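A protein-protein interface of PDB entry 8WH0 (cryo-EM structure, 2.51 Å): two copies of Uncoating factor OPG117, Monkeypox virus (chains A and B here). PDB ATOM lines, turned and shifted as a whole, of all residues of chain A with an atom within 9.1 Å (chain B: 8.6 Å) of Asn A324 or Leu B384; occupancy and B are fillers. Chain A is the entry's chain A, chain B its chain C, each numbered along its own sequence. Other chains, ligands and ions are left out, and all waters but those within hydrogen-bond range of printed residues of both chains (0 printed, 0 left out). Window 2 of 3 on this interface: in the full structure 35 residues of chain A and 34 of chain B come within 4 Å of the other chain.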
ATOM      1  N   GLY A 323      20.741  19.996  37.853  1.00  0.00           N
ATOM      2  CA  GLY A 323      20.243  18.753  37.294  1.00  0.00           C
ATOM      3  C   GLY A 323      19.686  18.903  35.894  1.00  0.00           C
ATOM      4  O   GLY A 323      18.475  18.849  35.691  1.00  0.00           O
ATOM      5  N   ASN A 324      20.578  19.084  34.919  1.00  0.00           N
ATOM      6  CA  ASN A 324      20.203  19.256  33.517  1.00  0.00           C
ATOM      7  C   ASN A 324      19.281  20.468  33.344  1.00  0.00           C
ATOM      8  O   ASN A 324      18.098  20.358  33.023  1.00  0.00           O
ATOM      9  CB  ASN A 324      19.565  17.981  32.958  1.00  0.00           C
ATOM     10  CG  ASN A 324      20.165  17.570  31.632  1.00  0.00           C
ATOM     11  OD1 ASN A 324      20.123  18.323  30.660  1.00  0.00           O
ATOM     12  ND2 ASN A 324      20.739  16.374  31.587  1.00  0.00           N
ATOM     13  N   LYS A 325      19.870  21.634  33.598  1.00  0.00           N
ATOM     14  CA  LYS A 325      19.201  22.923  33.454  1.00  0.00           C
ATOM     15  C   LYS A 325      18.320  23.006  32.211  1.00  0.00           C
ATOM     16  O   LYS A 325      17.213  23.551  32.268  1.00  0.00           O
ATOM     17  CB  LYS A 325      20.244  24.041  33.419  1.00  0.00           C
ATOM     18  CG  LYS A 325      19.674  25.430  33.610  1.00  0.00           C
ATOM     19  CD  LYS A 325      20.689  26.491  33.234  1.00  0.00           C
ATOM     20  CE  LYS A 325      21.987  26.309  34.002  1.00  0.00           C
ATOM     21  NZ  LYS A 325      22.057  27.203  35.187  1.00  0.00           N
ATOM     22  N   LEU A 326      18.799  22.478  31.083  1.00  0.00           N
ATOM     23  CA  LEU A 326      18.025  22.571  29.849  1.00  0.00           C
ATOM     24  C   LEU A 326      16.762  21.721  29.914  1.00  0.00           C
ATOM     25  O   LEU A 326      15.710  22.133  29.407  1.00  0.00           O
ATOM     26  CB  LEU A 326      18.891  22.167  28.657  1.00  0.00           C
ATOM     27  CG  LEU A 326      20.023  23.139  28.305  1.00  0.00           C
ATOM     28  CD1 LEU A 326      20.682  22.757  26.993  1.00  0.00           C
ATOM     29  CD2 LEU A 326      19.530  24.576  28.262  1.00  0.00           C
ATOM     30  N   PHE A 327      16.836  20.550  30.550  1.00  0.00           N
ATOM     31  CA  PHE A 327      15.633  19.755  30.762  1.00  0.00           C
ATOM     32  C   PHE A 327      14.645  20.485  31.662  1.00  0.00           C
ATOM     33  O   PHE A 327      13.433  20.416  31.444  1.00  0.00           O
ATOM     34  CB  PHE A 327      15.988  18.392  31.352  1.00  0.00           C
ATOM     35  CG  PHE A 327      14.876  17.388  31.255  1.00  0.00           C
ATOM     36  CD1 PHE A 327      14.629  16.725  30.068  1.00  0.00           C
ATOM     37  CD2 PHE A 327      14.067  17.123  32.345  1.00  0.00           C
ATOM     38  CE1 PHE A 327      13.605  15.810  29.974  1.00  0.00           C
ATOM     39  CE2 PHE A 327      13.042  16.211  32.254  1.00  0.00           C
ATOM     40  CZ  PHE A 327      12.811  15.553  31.070  1.00  0.00           C
ATOM     41  N   ASN A 328      15.143  21.183  32.685  1.00  0.00           N
ATOM     42  CA  ASN A 328      14.257  21.956  33.548  1.00  0.00           C
ATOM     43  C   ASN A 328      13.580  23.082  32.777  1.00  0.00           C
ATOM     44  O   ASN A 328      12.391  23.360  32.981  1.00  0.00           O
ATOM     45  CB  ASN A 328      15.041  22.512  34.737  1.00  0.00           C
ATOM     46  CG  ASN A 328      15.547  21.422  35.660  1.00  0.00           C
ATOM     47  OD1 ASN A 328      15.040  20.302  35.654  1.00  0.00           O
ATOM     48  ND2 ASN A 328      16.554  21.746  36.460  1.00  0.00           N
ATOM     49  N   ILE A 329      14.321  23.744  31.887  1.00  0.00           N
ATOM     50  CA  ILE A 329      13.729  24.790  31.057  1.00  0.00           C
ATOM     51  C   ILE A 329      12.629  24.207  30.179  1.00  0.00           C
ATOM     52  O   ILE A 329      11.542  24.783  30.043  1.00  0.00           O
ATOM     53  CB  ILE A 329      14.813  25.484  30.213  1.00  0.00           C
ATOM     54  CG1 ILE A 329      15.822  26.194  31.114  1.00  0.00           C
ATOM     55  CG2 ILE A 329      14.180  26.465  29.239  1.00  0.00           C
ATOM     56  CD1 ILE A 329      17.015  26.741  30.373  1.00  0.00           C
ATOM     57  N   ALA A 330      12.903  23.057  29.559  1.00  0.00           N
ATOM     58  CA  ALA A 330      11.888  22.407  28.737  1.00  0.00           C
ATOM     59  C   ALA A 330      10.662  22.038  29.564  1.00  0.00           C
ATOM     60  O   ALA A 330       9.525  22.182  29.103  1.00  0.00           O
ATOM     61  CB  ALA A 330      12.474  21.172  28.059  1.00  0.00           C
ATOM     62  N   GLN A 331      10.879  21.555  30.789  1.00  0.00           N
ATOM     63  CA  GLN A 331       9.770  21.198  31.666  1.00  0.00           C
ATOM     64  C   GLN A 331       8.904  22.411  31.980  1.00  0.00           C
ATOM     65  O   GLN A 331       7.671  22.333  31.952  1.00  0.00           O
ATOM     66  CB  GLN A 331      10.311  20.580  32.956  1.00  0.00           C
ATOM     67  CG  GLN A 331       9.931  19.132  33.172  1.00  0.00           C
ATOM     68  CD  GLN A 331       8.437  18.936  33.260  1.00  0.00           C
ATOM     69  OE1 GLN A 331       7.749  19.654  33.983  1.00  0.00           O
ATOM     70  NE2 GLN A 331       7.926  17.961  32.522  1.00  0.00           N
ATOM     71  N   TYR A 379      17.945  31.157  33.940  1.00  0.00           N
ATOM     72  CA  TYR A 379      17.454  30.335  32.842  1.00  0.00           C
ATOM     73  C   TYR A 379      17.347  31.120  31.542  1.00  0.00           C
ATOM     74  O   TYR A 379      17.508  30.543  30.462  1.00  0.00           O
ATOM     75  CB  TYR A 379      16.096  29.732  33.201  1.00  0.00           C
ATOM     76  CG  TYR A 379      16.183  28.536  34.118  1.00  0.00           C
ATOM     77  CD1 TYR A 379      17.399  28.131  34.645  1.00  0.00           C
ATOM     78  CD2 TYR A 379      15.052  27.808  34.451  1.00  0.00           C
ATOM     79  CE1 TYR A 379      17.486  27.041  35.480  1.00  0.00           C
ATOM     80  CE2 TYR A 379      15.131  26.714  35.285  1.00  0.00           C
ATOM     81  CZ  TYR A 379      16.351  26.335  35.797  1.00  0.00           C
ATOM     82  OH  TYR A 379      16.439  25.244  36.630  1.00  0.00           O
ATOM     83  N   GLU A 382      20.521  31.274  29.154  1.00  0.00           N
ATOM     84  CA  GLU A 382      20.870  30.082  28.393  1.00  0.00           C
ATOM     85  C   GLU A 382      20.222  30.064  27.017  1.00  0.00           C
ATOM     86  O   GLU A 382      20.738  29.404  26.111  1.00  0.00           O
ATOM     87  CB  GLU A 382      20.465  28.824  29.164  1.00  0.00           C
ATOM     88  CG  GLU A 382      21.282  28.567  30.411  1.00  0.00           C
ATOM     89  CD  GLU A 382      22.521  27.747  30.127  1.00  0.00           C
ATOM     90  OE1 GLU A 382      22.405  26.509  30.014  1.00  0.00           O
ATOM     91  OE2 GLU A 382      23.614  28.341  30.013  1.00  0.00           O
ATOM     92  N   THR A 391      18.514  22.116  21.706  1.00  0.00           N
ATOM     93  CA  THR A 391      18.461  21.064  22.719  1.00  0.00           C
ATOM     94  C   THR A 391      17.136  21.094  23.476  1.00  0.00           C
ATOM     95  O   THR A 391      16.505  20.052  23.708  1.00  0.00           O
ATOM     96  CB  THR A 391      19.634  21.210  23.689  1.00  0.00           C
ATOM     97  OG1 THR A 391      20.867  21.079  22.976  1.00  0.00           O
ATOM     98  CG2 THR A 391      19.573  20.145  24.766  1.00  0.00           C
ATOM     99  N   VAL A 392      16.699  22.290  23.875  1.00  0.00           N
ATOM    100  CA  VAL A 392      15.426  22.424  24.578  1.00  0.00           C
ATOM    101  C   VAL A 392      14.277  21.978  23.686  1.00  0.00           C
ATOM    102  O   VAL A 392      13.314  21.359  24.150  1.00  0.00           O
ATOM    103  CB  VAL A 392      15.239  23.872  25.070  1.00  0.00           C
ATOM    104  CG1 VAL A 392      13.832  24.081  25.590  1.00  0.00           C
ATOM    105  CG2 VAL A 392      16.259  24.200  26.141  1.00  0.00           C
ATOM    106  N   ALA A 394      14.441  19.689  21.316  1.00  0.00           N
ATOM    107  CA  ALA A 394      14.461  18.229  21.296  1.00  0.00           C
ATOM    108  C   ALA A 394      13.811  17.652  22.547  1.00  0.00           C
ATOM    109  O   ALA A 394      13.019  16.701  22.469  1.00  0.00           O
ATOM    110  CB  ALA A 394      15.896  17.724  21.156  1.00  0.00           C
ATOM    111  N   ASN A 395      14.124  18.223  23.712  1.00  0.00           N
ATOM    112  CA  ASN A 395      13.487  17.763  24.945  1.00  0.00           C
ATOM    113  C   ASN A 395      11.973  17.932  24.876  1.00  0.00           C
ATOM    114  O   ASN A 395      11.215  17.024  25.241  1.00  0.00           O
ATOM    115  CB  ASN A 395      14.057  18.514  26.146  1.00  0.00           C
ATOM    116  CG  ASN A 395      15.451  18.063  26.506  1.00  0.00           C
ATOM    117  OD1 ASN A 395      15.800  16.899  26.330  1.00  0.00           O
ATOM    118  ND2 ASN A 395      16.256  18.980  27.022  1.00  0.00           N
ATOM    119  N   ILE A 396      11.514  19.089  24.397  1.00  0.00           N
ATOM    120  CA  ILE A 396      10.079  19.348  24.306  1.00  0.00           C
ATOM    121  C   ILE A 396       9.416  18.361  23.354  1.00  0.00           C
ATOM    122  O   ILE A 396       8.323  17.853  23.626  1.00  0.00           O
ATOM    123  CB  ILE A 396       9.826  20.806  23.876  1.00  0.00           C
ATOM    124  CG1 ILE A 396       9.891  21.735  25.087  1.00  0.00           C
ATOM    125  CG2 ILE A 396       8.483  20.935  23.175  1.00  0.00           C
ATOM    126  CD1 ILE A 396      10.147  23.177  24.737  1.00  0.00           C
ATOM    127  N   ASP A 398      10.376  15.335  22.653  1.00  0.00           N
ATOM    128  CA  ASP A 398      10.275  14.044  23.323  1.00  0.00           C
ATOM    129  C   ASP A 398       9.231  14.044  24.434  1.00  0.00           C
ATOM    130  O   ASP A 398       8.715  12.977  24.778  1.00  0.00           O
ATOM    131  CB  ASP A 398      11.631  13.628  23.889  1.00  0.00           C
ATOM    132  CG  ASP A 398      12.556  13.073  22.829  1.00  0.00           C
ATOM    133  OD1 ASP A 398      12.062  12.679  21.753  1.00  0.00           O
ATOM    134  OD2 ASP A 398      13.781  13.033  23.069  1.00  0.00           O
ATOM    135  N   MET A 399       8.910  15.208  25.003  1.00  0.00           N
ATOM    136  CA  MET A 399       7.931  15.260  26.085  1.00  0.00           C
ATOM    137  C   MET A 399       6.490  15.169  25.593  1.00  0.00           C
ATOM    138  O   MET A 399       5.624  14.690  26.332  1.00  0.00           O
ATOM    139  CB  MET A 399       8.102  16.544  26.893  1.00  0.00           C
ATOM    140  CG  MET A 399       9.229  16.513  27.900  1.00  0.00           C
ATOM    141  SD  MET A 399       9.635  18.178  28.454  1.00  0.00           S
ATOM    142  CE  MET A 399      11.050  17.855  29.493  1.00  0.00           C
ATOM    143  N   ILE B 329      21.843   0.454  29.503  1.00  0.00           N
ATOM    144  CA  ILE B 329      20.509   1.050  29.519  1.00  0.00           C
ATOM    145  C   ILE B 329      19.670   0.505  28.369  1.00  0.00           C
ATOM    146  O   ILE B 329      18.489   0.171  28.542  1.00  0.00           O
ATOM    147  CB  ILE B 329      20.611   2.586  29.470  1.00  0.00           C
ATOM    148  CG1 ILE B 329      21.343   3.108  30.706  1.00  0.00           C
ATOM    149  CG2 ILE B 329      19.233   3.209  29.366  1.00  0.00           C
ATOM    150  CD1 ILE B 329      21.663   4.581  30.651  1.00  0.00           C
ATOM    151  N   ILE B 368      12.160   6.129  25.650  1.00  0.00           N
ATOM    152  CA  ILE B 368      13.307   6.194  26.553  1.00  0.00           C
ATOM    153  C   ILE B 368      13.061   7.235  27.638  1.00  0.00           C
ATOM    154  O   ILE B 368      13.258   6.980  28.837  1.00  0.00           O
ATOM    155  CB  ILE B 368      14.594   6.491  25.761  1.00  0.00           C
ATOM    156  CG1 ILE B 368      14.896   5.353  24.786  1.00  0.00           C
ATOM    157  CG2 ILE B 368      15.767   6.706  26.696  1.00  0.00           C
ATOM    158  CD1 ILE B 368      15.844   5.734  23.677  1.00  0.00           C
ATOM    159  N   LEU B 369      12.599   8.420  27.233  1.00  0.00           N
ATOM    160  CA  LEU B 369      12.347   9.485  28.195  1.00  0.00           C
ATOM    161  C   LEU B 369      11.241   9.104  29.172  1.00  0.00           C
ATOM    162  O   LEU B 369      11.324   9.415  30.365  1.00  0.00           O
ATOM    163  CB  LEU B 369      11.999  10.781  27.464  1.00  0.00           C
ATOM    164  CG  LEU B 369      12.065  12.063  28.295  1.00  0.00           C
ATOM    165  CD1 LEU B 369      13.385  12.164  29.034  1.00  0.00           C
ATOM    166  CD2 LEU B 369      11.854  13.276  27.413  1.00  0.00           C
ATOM    167  N   SER B 370      10.193   8.436  28.688  1.00  0.00           N
ATOM    168  CA  SER B 370       9.084   8.080  29.568  1.00  0.00           C
ATOM    169  C   SER B 370       9.442   6.933  30.504  1.00  0.00           C
ATOM    170  O   SER B 370       8.930   6.869  31.627  1.00  0.00           O
ATOM    171  CB  SER B 370       7.850   7.724  28.738  1.00  0.00           C
ATOM    172  OG  SER B 370       7.931   6.404  28.237  1.00  0.00           O
ATOM    173  N   ARG B 372      12.544   6.207  31.652  1.00  0.00           N
ATOM    174  CA  ARG B 372      13.661   6.492  32.548  1.00  0.00           C
ATOM    175  C   ARG B 372      13.332   6.259  34.021  1.00  0.00           C
ATOM    176  O   ARG B 372      14.252   6.064  34.824  1.00  0.00           O
ATOM    177  CB  ARG B 372      14.129   7.935  32.350  1.00  0.00           C
ATOM    178  CG  ARG B 372      13.400   8.956  33.202  1.00  0.00           C
ATOM    179  CD  ARG B 372      13.963  10.343  32.965  1.00  0.00           C
ATOM    180  NE  ARG B 372      13.272  11.374  33.730  1.00  0.00           N
ATOM    181  CZ  ARG B 372      12.131  11.941  33.364  1.00  0.00           C
ATOM    182  NH1 ARG B 372      11.499  11.576  32.263  1.00  0.00           N
ATOM    183  NH2 ARG B 372      11.610  12.898  34.125  1.00  0.00           N
ATOM    184  N   HIS B 373      12.055   6.280  34.406  1.00  0.00           N
ATOM    185  CA  HIS B 373      11.707   6.155  35.819  1.00  0.00           C
ATOM    186  C   HIS B 373      11.898   4.741  36.356  1.00  0.00           C
ATOM    187  O   HIS B 373      12.212   4.574  37.539  1.00  0.00           O
ATOM    188  CB  HIS B 373      10.264   6.603  36.047  1.00  0.00           C
ATOM    189  CG  HIS B 373      10.067   8.082  35.932  1.00  0.00           C
ATOM    190  ND1 HIS B 373      10.798   8.989  36.666  1.00  0.00           N
ATOM    191  CD2 HIS B 373       9.224   8.812  35.164  1.00  0.00           C
ATOM    192  CE1 HIS B 373      10.413  10.215  36.358  1.00  0.00           C
ATOM    193  NE2 HIS B 373       9.459  10.135  35.450  1.00  0.00           N
ATOM    194  N   TYR B 379      21.081   5.401  36.232  1.00  0.00           N
ATOM    195  CA  TYR B 379      20.815   5.304  34.802  1.00  0.00           C
ATOM    196  C   TYR B 379      19.822   6.356  34.325  1.00  0.00           C
ATOM    197  O   TYR B 379      19.853   6.739  33.150  1.00  0.00           O
ATOM    198  CB  TYR B 379      20.298   3.906  34.460  1.00  0.00           C
ATOM    199  CG  TYR B 379      21.372   2.844  34.450  1.00  0.00           C
ATOM    200  CD1 TYR B 379      22.710   3.181  34.586  1.00  0.00           C
ATOM    201  CD2 TYR B 379      21.047   1.504  34.303  1.00  0.00           C
ATOM    202  CE1 TYR B 379      23.693   2.215  34.577  1.00  0.00           C
ATOM    203  CE2 TYR B 379      22.024   0.530  34.292  1.00  0.00           C
ATOM    204  CZ  TYR B 379      23.345   0.891  34.430  1.00  0.00           C
ATOM    205  OH  TYR B 379      24.322  -0.076  34.420  1.00  0.00           O
ATOM    206  N   SER B 380      18.942   6.832  35.207  1.00  0.00           N
ATOM    207  CA  SER B 380      17.886   7.743  34.780  1.00  0.00           C
ATOM    208  C   SER B 380      18.418   9.139  34.480  1.00  0.00           C
ATOM    209  O   SER B 380      17.880   9.828  33.607  1.00  0.00           O
ATOM    210  CB  SER B 380      16.794   7.813  35.846  1.00  0.00           C
ATOM    211  OG  SER B 380      17.277   8.422  37.029  1.00  0.00           O
ATOM    212  N   SER B 381      19.464   9.576  35.185  1.00  0.00           N
ATOM    213  CA  SER B 381      19.979  10.925  34.983  1.00  0.00           C
ATOM    214  C   SER B 381      20.658  11.093  33.630  1.00  0.00           C
ATOM    215  O   SER B 381      20.759  12.222  33.140  1.00  0.00           O
ATOM    216  CB  SER B 381      20.953  11.288  36.104  1.00  0.00           C
ATOM    217  OG  SER B 381      22.143  10.525  36.014  1.00  0.00           O
ATOM    218  N   GLU B 382      21.127  10.004  33.021  1.00  0.00           N
ATOM    219  CA  GLU B 382      21.743  10.093  31.703  1.00  0.00           C
ATOM    220  C   GLU B 382      20.718  10.281  30.595  1.00  0.00           C
ATOM    221  O   GLU B 382      21.072  10.760  29.515  1.00  0.00           O
ATOM    222  CB  GLU B 382      22.577   8.842  31.426  1.00  0.00           C
ATOM    223  CG  GLU B 382      23.526   8.468  32.547  1.00  0.00           C
ATOM    224  CD  GLU B 382      24.953   8.892  32.265  1.00  0.00           C
ATOM    225  OE1 GLU B 382      25.478   8.538  31.189  1.00  0.00           O
ATOM    226  OE2 GLU B 382      25.549   9.580  33.118  1.00  0.00           O
ATOM    227  N   LEU B 383      19.461   9.928  30.841  1.00  0.00           N
ATOM    228  CA  LEU B 383      18.435   9.968  29.811  1.00  0.00           C
ATOM    229  C   LEU B 383      17.818  11.348  29.633  1.00  0.00           C
ATOM    230  O   LEU B 383      16.927  11.504  28.793  1.00  0.00           O
ATOM    231  CB  LEU B 383      17.345   8.944  30.127  1.00  0.00           C
ATOM    232  CG  LEU B 383      17.837   7.498  30.196  1.00  0.00           C
ATOM    233  CD1 LEU B 383      16.693   6.557  30.519  1.00  0.00           C
ATOM    234  CD2 LEU B 383      18.508   7.105  28.893  1.00  0.00           C
ATOM    235  N   LEU B 384      18.258  12.344  30.402  1.00  0.00           N
ATOM    236  CA  LEU B 384      17.790  13.711  30.218  1.00  0.00           C
ATOM    237  C   LEU B 384      18.507  14.433  29.085  1.00  0.00           C
ATOM    238  O   LEU B 384      18.109  15.548  28.735  1.00  0.00           O
ATOM    239  CB  LEU B 384      17.957  14.500  31.518  1.00  0.00           C
ATOM    240  CG  LEU B 384      17.248  13.940  32.753  1.00  0.00           C
ATOM    241  CD1 LEU B 384      17.372  14.895  33.921  1.00  0.00           C
ATOM    242  CD2 LEU B 384      15.793  13.660  32.451  1.00  0.00           C
ATOM    243  N   CYS B 385      19.546  13.829  28.507  1.00  0.00           N
ATOM    244  CA  CYS B 385      20.272  14.421  27.394  1.00  0.00           C
ATOM    245  C   CYS B 385      19.757  13.848  26.086  1.00  0.00           C
ATOM    246  O   CYS B 385      19.754  12.619  25.922  1.00  0.00           O
ATOM    247  CB  CYS B 385      21.766  14.158  27.533  1.00  0.00           C
ATOM    248  SG  CYS B 385      22.799  14.973  26.293  1.00  0.00           S
ATOM    249  N   PRO B 386      19.309  14.674  25.139  1.00  0.00           N
ATOM    250  CA  PRO B 386      18.832  14.125  23.859  1.00  0.00           C
ATOM    251  C   PRO B 386      19.886  13.328  23.105  1.00  0.00           C
ATOM    252  O   PRO B 386      19.542  12.362  22.413  1.00  0.00           O
ATOM    253  CB  PRO B 386      18.400  15.373  23.076  1.00  0.00           C
ATOM    254  CG  PRO B 386      18.281  16.463  24.083  1.00  0.00           C
ATOM    255  CD  PRO B 386      19.213  16.141  25.196  1.00  0.00           C
ATOM    256  N   ARG B 387      21.160  13.711  23.210  1.00  0.00           N
ATOM    257  CA  ARG B 387      22.222  12.978  22.528  1.00  0.00           C
ATOM    258  C   ARG B 387      22.389  11.572  23.097  1.00  0.00           C
ATOM    259  O   ARG B 387      22.545  10.600  22.344  1.00  0.00           O
ATOM    260  CB  ARG B 387      23.527  13.767  22.625  1.00  0.00           C
ATOM    261  CG  ARG B 387      24.657  13.239  21.763  1.00  0.00           C
ATOM    262  CD  ARG B 387      25.995  13.402  22.467  1.00  0.00           C
ATOM    263  NE  ARG B 387      26.260  12.320  23.408  1.00  0.00           N
ATOM    264  CZ  ARG B 387      26.427  11.050  23.066  1.00  0.00           C
ATOM    265  NH1 ARG B 387      26.383  10.663  21.802  1.00  0.00           N
ATOM    266  NH2 ARG B 387      26.648  10.147  24.016  1.00  0.00           N
ATOM    267  N   LYS B 388      22.358  11.443  24.424  1.00  0.00           N
ATOM    268  CA  LYS B 388      22.430  10.123  25.038  1.00  0.00           C
ATOM    269  C   LYS B 388      21.231   9.274  24.642  1.00  0.00           C
ATOM    270  O   LYS B 388      21.362   8.065  24.416  1.00  0.00           O
ATOM    271  CB  LYS B 388      22.514  10.254  26.558  1.00  0.00           C
ATOM    272  CG  LYS B 388      23.562  11.235  27.039  1.00  0.00           C
ATOM    273  CD  LYS B 388      24.911  10.567  27.196  1.00  0.00           C
ATOM    274  CE  LYS B 388      25.787  11.315  28.182  1.00  0.00           C
ATOM    275  NZ  LYS B 388      25.005  11.834  29.334  1.00  0.00           N
ATOM    276  N   ARG B 389      20.051   9.888  24.561  1.00  0.00           N
ATOM    277  CA  ARG B 389      18.869   9.159  24.122  1.00  0.00           C
ATOM    278  C   ARG B 389      19.019   8.682  22.684  1.00  0.00           C
ATOM    279  O   ARG B 389      18.598   7.572  22.347  1.00  0.00           O
ATOM    280  CB  ARG B 389      17.625  10.030  24.283  1.00  0.00           C
ATOM    281  CG  ARG B 389      17.326  10.404  25.723  1.00  0.00           C
ATOM    282  CD  ARG B 389      15.872  10.793  25.913  1.00  0.00           C
ATOM    283  NE  ARG B 389      15.524  12.008  25.187  1.00  0.00           N
ATOM    284  CZ  ARG B 389      15.563  13.227  25.705  1.00  0.00           C
ATOM    285  NH1 ARG B 389      15.933  13.436  26.956  1.00  0.00           N
ATOM    286  NH2 ARG B 389      15.219  14.264  24.946  1.00  0.00           N
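The side-chain amide nitrogen (ND2) of Asn A395 is in hydrogen-bond range of the backbone carbonyl oxygen (O) of Thr A391 (3.5 Å).
The backbone carbonyl oxygen of Leu B369 lies within hydrogen-bond range of the guanidinium group of Arg B372 (2.9 Å).
The backbone carbonyl oxygen of Leu B383 sits at hydrogen-bond distance from the guanidinium group of Arg B389, 2.8 Å away.
Positions printed for both chains: 329, 379 and 382.
CB of Leu B384 touches ND2 of Asn A324 (3.4 Å).
Leu B369 touches Phe A327 (CD1 to CE1, 3.8 Å).
CE2 of Phe A327 touches CD2 of Leu B384, at 3.8 Å.
CG2 of Thr A391 touches CG of Pro B386, 3.96 Å away.
CB of Ala A394 touches CB of Pro B386, at 3.9 Å.
Leu B384 touches Asn A395.
CG of Pro B386 touches OD1 of Asn A395 (3.4 Å).
CD2 of Leu B369 touches CB of Asp A398, at 3.5 Å.
OD1 of Asn A395 sits at hydrogen-bond distance from NH2 of Arg B389.
NH2 of Arg B389 is in salt-bridge range of OD2 of Asp A398 (2.7 Å).
Asn A324 touches just one residue of chain B: Leu B384 (3.4 Å).
Of the printed residues of chain A, Leu B384 touches Asn A324, Phe A327 and Asn A395.
No residue of chain B comes within 4 Å of Gly A323.
Of the printed residues of chain B, Asp A398 touches Leu B369 (3.5 Å) and Arg B389 (2.7 Å).
Of the printed residues of chain A, Leu B369 touches Phe A327 and Asp A398.
Of the printed residues of chain A, Pro B386 touches Thr A391, Ala A394 and Asn A395.
Of the printed residues of chain B, Ala A394 touches Pro B386 (3.9 Å).
Ala A330 touches none of the printed residues of chain B.
The nearest printed residue of chain B that does not touch Ala A394 is Arg B389 (4.1 Å).
Of the 17 printed residues of chain B, 4 touch a printed residue of chain A.
Hydrophobic or aromatic side chains of chain B within 4 Å of the printed part of chain A: Leu B369, Leu B384 and Pro B386.
Among the printed residues, 10 pairs touch across the chains.
Among the printed residues, Asp or Glu carboxylates within 4 Å of a Lys or Arg side-chain nitrogen of the other chain: Asp A398 with Arg B389.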
